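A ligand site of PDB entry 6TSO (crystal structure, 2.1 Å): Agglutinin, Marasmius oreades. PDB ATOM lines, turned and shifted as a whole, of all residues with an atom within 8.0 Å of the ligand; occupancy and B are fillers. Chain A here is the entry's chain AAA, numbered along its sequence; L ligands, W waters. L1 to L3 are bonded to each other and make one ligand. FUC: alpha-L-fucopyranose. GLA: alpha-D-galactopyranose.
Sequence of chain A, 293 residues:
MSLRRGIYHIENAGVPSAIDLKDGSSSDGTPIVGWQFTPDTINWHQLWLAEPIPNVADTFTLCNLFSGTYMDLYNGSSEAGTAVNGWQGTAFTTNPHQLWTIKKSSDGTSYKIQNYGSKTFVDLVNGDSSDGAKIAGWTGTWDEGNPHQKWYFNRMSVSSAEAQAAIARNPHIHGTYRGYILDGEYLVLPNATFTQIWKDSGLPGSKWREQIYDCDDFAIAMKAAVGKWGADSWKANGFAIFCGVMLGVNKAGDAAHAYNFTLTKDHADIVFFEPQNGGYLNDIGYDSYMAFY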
ATOM      1  N   ASP A  28       5.271  -8.786  -8.616  1.00  0.00           N
ATOM      2  CA  ASP A  28       5.030  -8.572  -7.169  1.00  0.00           C
ATOM      3  C   ASP A  28       3.525  -8.690  -6.910  1.00  0.00           C
ATOM      4  O   ASP A  28       2.759  -8.111  -7.712  1.00  0.00           O
ATOM      5  CB  ASP A  28       5.559  -7.217  -6.698  1.00  0.00           C
ATOM      6  CG  ASP A  28       7.062  -7.096  -6.607  1.00  0.00           C
ATOM      7  OD1 ASP A  28       7.748  -8.164  -6.555  1.00  0.00           O
ATOM      8  OD2 ASP A  28       7.548  -5.924  -6.540  1.00  0.00           O
ATOM      9  N   GLY A  29       3.120  -9.456  -5.893  1.00  0.00           N
ATOM     10  CA  GLY A  29       1.695  -9.617  -5.539  1.00  0.00           C
ATOM     11  C   GLY A  29       0.987 -10.688  -6.378  1.00  0.00           C
ATOM     12  O   GLY A  29      -0.256 -10.805  -6.290  1.00  0.00           O
ATOM     13  N   TYR A  70       9.674 -14.631  -3.838  1.00  0.00           N
ATOM     14  CA  TYR A  70       9.597 -15.186  -2.468  1.00  0.00           C
ATOM     15  C   TYR A  70       8.147 -15.212  -2.012  1.00  0.00           C
ATOM     16  O   TYR A  70       7.414 -14.286  -2.347  1.00  0.00           O
ATOM     17  CB  TYR A  70      10.497 -14.343  -1.550  1.00  0.00           C
ATOM     18  CG  TYR A  70      11.947 -14.581  -1.872  1.00  0.00           C
ATOM     19  CD1 TYR A  70      12.571 -13.832  -2.854  1.00  0.00           C
ATOM     20  CD2 TYR A  70      12.666 -15.598  -1.243  1.00  0.00           C
ATOM     21  CE1 TYR A  70      13.890 -14.077  -3.200  1.00  0.00           C
ATOM     22  CE2 TYR A  70      13.985 -15.841  -1.572  1.00  0.00           C
ATOM     23  CZ  TYR A  70      14.598 -15.071  -2.546  1.00  0.00           C
ATOM     24  OH  TYR A  70      15.874 -15.290  -2.926  1.00  0.00           O
ATOM     25  N   MET A  71       7.765 -16.264  -1.289  1.00  0.00           N
ATOM     26  CA  MET A  71       6.471 -16.339  -0.555  1.00  0.00           C
ATOM     27  C   MET A  71       6.416 -15.198   0.466  1.00  0.00           C
ATOM     28  O   MET A  71       7.300 -15.082   1.314  1.00  0.00           O
ATOM     29  CB  MET A  71       6.317 -17.662   0.184  1.00  0.00           C
ATOM     30  CG  MET A  71       4.968 -17.834   0.839  1.00  0.00           C
ATOM     31  SD  MET A  71       4.803 -19.444   1.540  1.00  0.00           S
ATOM     32  CE  MET A  71       4.858 -20.429   0.039  1.00  0.00           C
ATOM     33  N   ASP A  72       5.394 -14.353   0.333  1.00  0.00           N
ATOM     34  CA  ASP A  72       5.288 -13.039   0.994  1.00  0.00           C
ATOM     35  C   ASP A  72       3.892 -12.923   1.575  1.00  0.00           C
ATOM     36  O   ASP A  72       2.890 -13.090   0.826  1.00  0.00           O
ATOM     37  CB  ASP A  72       5.557 -11.895   0.027  1.00  0.00           C
ATOM     38  CG  ASP A  72       5.473 -10.540   0.711  1.00  0.00           C
ATOM     39  OD1 ASP A  72       4.376 -10.081   0.934  1.00  0.00           O
ATOM     40  OD2 ASP A  72       6.519  -9.986   1.027  1.00  0.00           O
ATOM     41  N   LEU A  73       3.833 -12.705   2.878  1.00  0.00           N
ATOM     42  CA  LEU A  73       2.576 -12.426   3.599  1.00  0.00           C
ATOM     43  C   LEU A  73       2.310 -10.923   3.493  1.00  0.00           C
ATOM     44  O   LEU A  73       3.167 -10.109   3.976  1.00  0.00           O
ATOM     45  CB  LEU A  73       2.706 -12.882   5.050  1.00  0.00           C
ATOM     46  CG  LEU A  73       1.489 -12.648   5.931  1.00  0.00           C
ATOM     47  CD1 LEU A  73       0.305 -13.491   5.476  1.00  0.00           C
ATOM     48  CD2 LEU A  73       1.821 -12.912   7.396  1.00  0.00           C
ATOM     49  N   TYR A  74       1.216 -10.580   2.834  1.00  0.00           N
ATOM     50  CA  TYR A  74       0.935  -9.193   2.359  1.00  0.00           C
ATOM     51  C   TYR A  74       0.914  -8.279   3.585  1.00  0.00           C
ATOM     52  O   TYR A  74       0.121  -8.537   4.501  1.00  0.00           O
ATOM     53  CB  TYR A  74      -0.377  -9.132   1.577  1.00  0.00           C
ATOM     54  CG  TYR A  74      -0.609  -7.796   0.918  1.00  0.00           C
ATOM     55  CD1 TYR A  74       0.282  -7.299  -0.010  1.00  0.00           C
ATOM     56  CD2 TYR A  74      -1.702  -7.004   1.248  1.00  0.00           C
ATOM     57  CE1 TYR A  74       0.098  -6.059  -0.612  1.00  0.00           C
ATOM     58  CE2 TYR A  74      -1.909  -5.771   0.646  1.00  0.00           C
ATOM     59  CZ  TYR A  74      -1.001  -5.291  -0.279  1.00  0.00           C
ATOM     60  OH  TYR A  74      -1.195  -4.101  -0.892  1.00  0.00           O
ATOM     61  N   ASN A  75       1.838  -7.328   3.622  1.00  0.00           N
ATOM     62  CA  ASN A  75       1.994  -6.275   4.666  1.00  0.00           C
ATOM     63  C   ASN A  75       2.250  -6.899   6.039  1.00  0.00           C
ATOM     64  O   ASN A  75       2.181  -6.147   7.044  1.00  0.00           O
ATOM     65  CB  ASN A  75       0.781  -5.343   4.703  1.00  0.00           C
ATOM     66  CG  ASN A  75       0.765  -4.380   3.533  1.00  0.00           C
ATOM     67  OD1 ASN A  75       1.807  -3.830   3.171  1.00  0.00           O
ATOM     68  ND2 ASN A  75      -0.394  -4.213   2.929  1.00  0.00           N
ATOM     69  N   GLY A  76       2.548  -8.210   6.070  1.00  0.00           N
ATOM     70  CA  GLY A  76       2.800  -8.977   7.302  1.00  0.00           C
ATOM     71  C   GLY A  76       1.623  -8.965   8.264  1.00  0.00           C
ATOM     72  O   GLY A  76       1.877  -9.154   9.459  1.00  0.00           O
ATOM     73  N   SER A  77       0.386  -8.797   7.776  1.00  0.00           N
ATOM     74  CA  SER A  77      -0.839  -8.708   8.609  1.00  0.00           C
ATOM     75  C   SER A  77      -1.107 -10.071   9.270  1.00  0.00           C
ATOM     76  O   SER A  77      -1.003 -11.115   8.574  1.00  0.00           O
ATOM     77  CB  SER A  77      -2.027  -8.232   7.794  1.00  0.00           C
ATOM     78  OG  SER A  77      -3.201  -8.246   8.585  1.00  0.00           O
ATOM     79  N   THR A  82      -5.417 -12.961   5.182  1.00  0.00           N
ATOM     80  CA  THR A  82      -4.332 -12.144   4.576  1.00  0.00           C
ATOM     81  C   THR A  82      -3.704 -12.898   3.404  1.00  0.00           C
ATOM     82  O   THR A  82      -3.337 -14.101   3.554  1.00  0.00           O
ATOM     83  CB  THR A  82      -3.267 -11.764   5.596  1.00  0.00           C
ATOM     84  OG1 THR A  82      -3.800 -10.940   6.642  1.00  0.00           O
ATOM     85  CG2 THR A  82      -2.126 -10.991   4.986  1.00  0.00           C
ATOM     86  N   ALA A  83      -3.515 -12.209   2.284  1.00  0.00           N
ATOM     87  CA  ALA A  83      -2.974 -12.758   1.016  1.00  0.00           C
ATOM     88  C   ALA A  83      -1.538 -13.260   1.231  1.00  0.00           C
ATOM     89  O   ALA A  83      -0.738 -12.560   1.912  1.00  0.00           O
ATOM     90  CB  ALA A  83      -3.047 -11.711  -0.075  1.00  0.00           C
ATOM     91  N   ASN A  85       1.465 -14.025  -1.347  1.00  0.00           N
ATOM     92  CA  ASN A  85       1.863 -13.726  -2.743  1.00  0.00           C
ATOM     93  C   ASN A  85       3.339 -14.025  -2.979  1.00  0.00           C
ATOM     94  O   ASN A  85       4.139 -14.097  -2.021  1.00  0.00           O
ATOM     95  CB  ASN A  85       1.602 -12.265  -3.123  1.00  0.00           C
ATOM     96  CG  ASN A  85       0.182 -11.838  -2.847  1.00  0.00           C
ATOM     97  OD1 ASN A  85      -0.766 -12.500  -3.280  1.00  0.00           O
ATOM     98  ND2 ASN A  85       0.024 -10.737  -2.108  1.00  0.00           N
ATOM     99  N   GLY A  86       3.676 -14.133  -4.271  1.00  0.00           N
ATOM    100  CA  GLY A  86       5.034 -13.952  -4.793  1.00  0.00           C
ATOM    101  C   GLY A  86       5.433 -12.491  -4.720  1.00  0.00           C
ATOM    102  O   GLY A  86       4.633 -11.617  -5.106  1.00  0.00           O
ATOM    103  N   TRP A  87       6.632 -12.215  -4.237  1.00  0.00           N
ATOM    104  CA  TRP A  87       7.162 -10.830  -4.091  1.00  0.00           C
ATOM    105  C   TRP A  87       8.664 -10.845  -4.289  1.00  0.00           C
ATOM    106  O   TRP A  87       9.279 -11.824  -3.872  1.00  0.00           O
ATOM    107  CB  TRP A  87       6.814 -10.242  -2.726  1.00  0.00           C
ATOM    108  CG  TRP A  87       6.615  -8.758  -2.800  1.00  0.00           C
ATOM    109  CD1 TRP A  87       7.575  -7.792  -2.829  1.00  0.00           C
ATOM    110  CD2 TRP A  87       5.370  -8.087  -2.886  1.00  0.00           C
ATOM    111  NE1 TRP A  87       6.997  -6.552  -2.947  1.00  0.00           N
ATOM    112  CE2 TRP A  87       5.642  -6.705  -2.966  1.00  0.00           C
ATOM    113  CE3 TRP A  87       4.043  -8.515  -2.939  1.00  0.00           C
ATOM    114  CZ2 TRP A  87       4.638  -5.747  -3.082  1.00  0.00           C
ATOM    115  CZ3 TRP A  87       3.042  -7.565  -3.019  1.00  0.00           C
ATOM    116  CH2 TRP A  87       3.344  -6.211  -3.100  1.00  0.00           C
ATOM    117  N   GLN A  88       9.218  -9.816  -4.924  1.00  0.00           N
ATOM    118  CA  GLN A  88      10.686  -9.671  -5.041  1.00  0.00           C
ATOM    119  C   GLN A  88      11.281  -9.680  -3.617  1.00  0.00           C
ATOM    120  O   GLN A  88      10.637  -9.178  -2.682  1.00  0.00           O
ATOM    121  CB  GLN A  88      11.069  -8.387  -5.770  1.00  0.00           C
ATOM    122  CG  GLN A  88      10.870  -7.102  -4.972  1.00  0.00           C
ATOM    123  CD  GLN A  88      11.243  -5.926  -5.843  1.00  0.00           C
ATOM    124  OE1 GLN A  88      12.417  -5.621  -6.024  1.00  0.00           O
ATOM    125  NE2 GLN A  88      10.242  -5.325  -6.464  1.00  0.00           N
ATOM    126  N   GLY A  89      12.457 -10.286  -3.454  1.00  0.00           N
ATOM    127  CA  GLY A  89      13.218 -10.269  -2.189  1.00  0.00           C
ATOM    128  C   GLY A  89      14.585 -10.876  -2.362  1.00  0.00           C
ATOM    129  O   GLY A  89      15.084 -10.839  -3.488  1.00  0.00           O
ATOM    130  N   THR A  90      15.177 -11.430  -1.298  1.00  0.00           N
ATOM    131  CA  THR A  90      16.520 -12.071  -1.309  1.00  0.00           C
ATOM    132  C   THR A  90      16.545 -13.222  -0.307  1.00  0.00           C
ATOM    133  O   THR A  90      15.677 -13.234   0.605  1.00  0.00           O
ATOM    134  CB  THR A  90      17.668 -11.118  -0.942  1.00  0.00           C
ATOM    135  OG1 THR A  90      17.392 -10.607   0.366  1.00  0.00           O
ATOM    136  CG2 THR A  90      17.843  -9.977  -1.932  1.00  0.00           C
ATOM    137  N   THR A  93      17.032 -12.269   3.432  1.00  0.00           N
ATOM    138  CA  THR A  93      16.274 -11.047   3.794  1.00  0.00           C
ATOM    139  C   THR A  93      15.942 -11.033   5.288  1.00  0.00           C
ATOM    140  O   THR A  93      15.727 -12.089   5.845  1.00  0.00           O
ATOM    141  CB  THR A  93      14.953 -10.928   3.014  1.00  0.00           C
ATOM    142  OG1 THR A  93      14.383  -9.657   3.319  1.00  0.00           O
ATOM    143  CG2 THR A  93      13.970 -12.026   3.350  1.00  0.00           C
ATOM    144  N   THR A  94      15.864  -9.836   5.857  1.00  0.00           N
ATOM    145  CA  THR A  94      15.337  -9.589   7.219  1.00  0.00           C
ATOM    146  C   THR A  94      13.871  -9.159   7.131  1.00  0.00           C
ATOM    147  O   THR A  94      13.283  -8.926   8.191  1.00  0.00           O
ATOM    148  CB  THR A  94      16.188  -8.524   7.926  1.00  0.00           C
ATOM    149  OG1 THR A  94      16.148  -7.374   7.089  1.00  0.00           O
ATOM    150  CG2 THR A  94      17.597  -9.012   8.192  1.00  0.00           C
ATOM    151  N   ASN A  95      13.288  -9.082   5.925  1.00  0.00           N
ATOM    152  CA  ASN A  95      11.842  -8.740   5.757  1.00  0.00           C
ATOM    153  C   ASN A  95      11.005  -9.886   6.307  1.00  0.00           C
ATOM    154  O   ASN A  95      10.988 -10.959   5.712  1.00  0.00           O
ATOM    155  CB  ASN A  95      11.479  -8.445   4.310  1.00  0.00           C
ATOM    156  CG  ASN A  95      10.015  -8.158   4.122  1.00  0.00           C
ATOM    157  OD1 ASN A  95       9.205  -8.261   5.055  1.00  0.00           O
ATOM    158  ND2 ASN A  95       9.662  -7.773   2.895  1.00  0.00           N
ATOM    159  N   PRO A  96      10.298  -9.715   7.444  1.00  0.00           N
ATOM    160  CA  PRO A  96       9.646 -10.856   8.089  1.00  0.00           C
ATOM    161  C   PRO A  96       8.368 -11.283   7.330  1.00  0.00           C
ATOM    162  O   PRO A  96       7.927 -12.345   7.586  1.00  0.00           O
ATOM    163  CB  PRO A  96       9.333 -10.378   9.542  1.00  0.00           C
ATOM    164  CG  PRO A  96       9.621  -8.870   9.565  1.00  0.00           C
ATOM    165  CD  PRO A  96      10.144  -8.458   8.213  1.00  0.00           C
ATOM    166  N   HIS A  97       7.868 -10.484   6.399  1.00  0.00           N
ATOM    167  CA  HIS A  97       6.776 -10.892   5.488  1.00  0.00           C
ATOM    168  C   HIS A  97       7.237 -12.112   4.683  1.00  0.00           C
ATOM    169  O   HIS A  97       6.387 -12.831   4.080  1.00  0.00           O
ATOM    170  CB  HIS A  97       6.357  -9.741   4.551  1.00  0.00           C
ATOM    171  CG  HIS A  97       6.068  -8.431   5.204  1.00  0.00           C
ATOM    172  ND1 HIS A  97       5.735  -7.305   4.459  1.00  0.00           N
ATOM    173  CD2 HIS A  97       6.112  -8.019   6.491  1.00  0.00           C
ATOM    174  CE1 HIS A  97       5.556  -6.284   5.252  1.00  0.00           C
ATOM    175  NE2 HIS A  97       5.791  -6.699   6.517  1.00  0.00           N
ATOM    176  N   GLN A  98       8.562 -12.282   4.565  1.00  0.00           N
ATOM    177  CA  GLN A  98       9.147 -13.326   3.683  1.00  0.00           C
ATOM    178  C   GLN A  98       9.874 -14.389   4.529  1.00  0.00           C
ATOM    179  O   GLN A  98      10.581 -15.216   3.931  1.00  0.00           O
ATOM    180  CB  GLN A  98      10.078 -12.636   2.673  1.00  0.00           C
ATOM    181  CG  GLN A  98       9.293 -11.838   1.634  1.00  0.00           C
ATOM    182  CD  GLN A  98      10.129 -11.162   0.578  1.00  0.00           C
ATOM    183  OE1 GLN A  98      11.339 -11.311   0.531  1.00  0.00           O
ATOM    184  NE2 GLN A  98       9.468 -10.431  -0.315  1.00  0.00           N
HETATM  185  C1  FUC L   1       9.642  -3.548   2.759  1.00  0.00           C
HETATM  186  C2  FUC L   1      10.425  -2.276   2.405  1.00  0.00           C
HETATM  187  C3  FUC L   1       9.697  -1.029   2.863  1.00  0.00           C
HETATM  188  C4  FUC L   1       9.311  -1.163   4.332  1.00  0.00           C
HETATM  189  C5  FUC L   1       8.435  -2.403   4.504  1.00  0.00           C
HETATM  190  C6  FUC L   1       7.968  -2.582   5.939  1.00  0.00           C
HETATM  191  O2  FUC L   1      10.614  -2.136   0.979  1.00  0.00           O
HETATM  192  O3  FUC L   1      10.582   0.078   2.635  1.00  0.00           O
HETATM  193  O4  FUC L   1      10.483  -1.222   5.165  1.00  0.00           O
HETATM  194  O5  FUC L   1       9.157  -3.567   4.110  1.00  0.00           O
HETATM  195  C1  GLA L   2       6.124  -4.339   2.332  1.00  0.00           C
HETATM  196  C2  GLA L   2       7.590  -4.747   2.089  1.00  0.00           C
HETATM  197  C3  GLA L   2       7.757  -5.464   0.735  1.00  0.00           C
HETATM  198  C4  GLA L   2       6.761  -6.670   0.690  1.00  0.00           C
HETATM  199  C5  GLA L   2       5.356  -6.058   0.780  1.00  0.00           C
HETATM  200  C6  GLA L   2       4.191  -7.039   0.651  1.00  0.00           C
HETATM  201  O1  GLA L   2       5.711  -3.269   1.483  1.00  0.00           O
HETATM  202  O2  GLA L   2       8.488  -3.626   2.117  1.00  0.00           O
HETATM  203  O3  GLA L   2       9.154  -5.780   0.542  1.00  0.00           O
HETATM  204  O4  GLA L   2       7.008  -7.640   1.696  1.00  0.00           O
HETATM  205  O5  GLA L   2       5.224  -5.433   2.055  1.00  0.00           O
HETATM  206  O6  GLA L   2       4.107  -7.859   1.827  1.00  0.00           O
HETATM  207  C1  GLA L   3       9.834  -6.301  -0.484  1.00  0.00           C
HETATM  208  C2  GLA L   3      11.337  -6.470  -0.383  1.00  0.00           C
HETATM  209  C3  GLA L   3      11.881  -5.045  -0.343  1.00  0.00           C
HETATM  210  C4  GLA L   3      11.463  -4.277  -1.577  1.00  0.00           C
HETATM  211  C5  GLA L   3       9.937  -4.289  -1.738  1.00  0.00           C
HETATM  212  C6  GLA L   3       9.467  -3.628  -3.033  1.00  0.00           C
HETATM  213  O2  GLA L   3      11.722  -7.249   0.753  1.00  0.00           O
HETATM  214  O3  GLA L   3      13.292  -5.087  -0.298  1.00  0.00           O
HETATM  215  O4  GLA L   3      12.140  -4.891  -2.665  1.00  0.00           O
HETATM  216  O5  GLA L   3       9.502  -5.635  -1.730  1.00  0.00           O
HETATM  217  O6  GLA L   3       8.045  -3.653  -3.143  1.00  0.00           O
HETATM  218  O   HOH W   1      12.978  -9.313   1.007  1.00  0.00           O
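A ring nitrogen (ND1) of His 97 sits at hydrogen-bond distance from an oxygen (O4) of GLA L2 (3.1 Å).
The side-chain amide oxygen (OE1) of Gln 88 lies close to an oxygen (O4) of GLA L3, at 3.4 Å.
An oxygen (O6) of GLA L2 lies within hydrogen-bond range of the backbone NH of Asn 75 (2.9 Å).
An oxygen (O4) of GLA L2 lies within hydrogen-bond range of the side-chain amide nitrogen (ND2) of Asn 95.
An oxygen (O5) of GLA L3 sits at hydrogen-bond distance from the indole nitrogen (NE1) of Trp 87.
An oxygen (O6) of GLA L2 is in hydrogen-bond range of the backbone carbonyl oxygen of Leu 73, 3.3 Å away.
The side-chain carboxylate (OD1) of Asp 72 lies within hydrogen-bond range of an oxygen (O6) of GLA L2.
CA of Tyr 74 touches O6 of GLA L2, 3.5 Å away.
Hydrophobic or aromatic side chains within 4 Å of the ligand: Tyr 74, Trp 87 and His 97.
Within 4 Å of the ligand: Asp 72, Leu 73, Tyr 74, Asn 75, Trp 87, Gln 88, Asn 95 and His 97.
Along chain A the residues within 4 Å of the ligand span positions 72 to 97.
Water W1 lies within hydrogen-bond range of O2 of GLA L3 (2.4 Å), OE1 of Gln 98 (2.6 Å) and OG1 of Thr 93 (2.7 Å).
The backbone carbonyl oxygen (O) of Trp 87 lies within hydrogen-bond range of the backbone NH (N) of Tyr 70 (2.8 Å).
The backbone NH of Asp 72 sits at hydrogen-bond distance from the backbone carbonyl oxygen of Asn 85, at 2.7 Å.
The side-chain amide nitrogen of Gln 98 sits at hydrogen-bond distance from the backbone carbonyl oxygen of Gln 88, at 2.9 Å.
N of Gln 88 sits at hydrogen-bond distance from OD1 of Asp 28.
The side-chain carboxylate of Asp 72 is in hydrogen-bond range of the side-chain amide nitrogen of Gln 98 (3.3 Å).
N of Asn 95 sits at hydrogen-bond distance from OG1 of Thr 93, at 2.9 Å.
The backbone NH of His 97 sits at hydrogen-bond distance from the side-chain amide oxygen of Asn 95, at 2.9 Å.
N of Tyr 74 is in hydrogen-bond range of O of Ala 83, 2.9 Å away.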
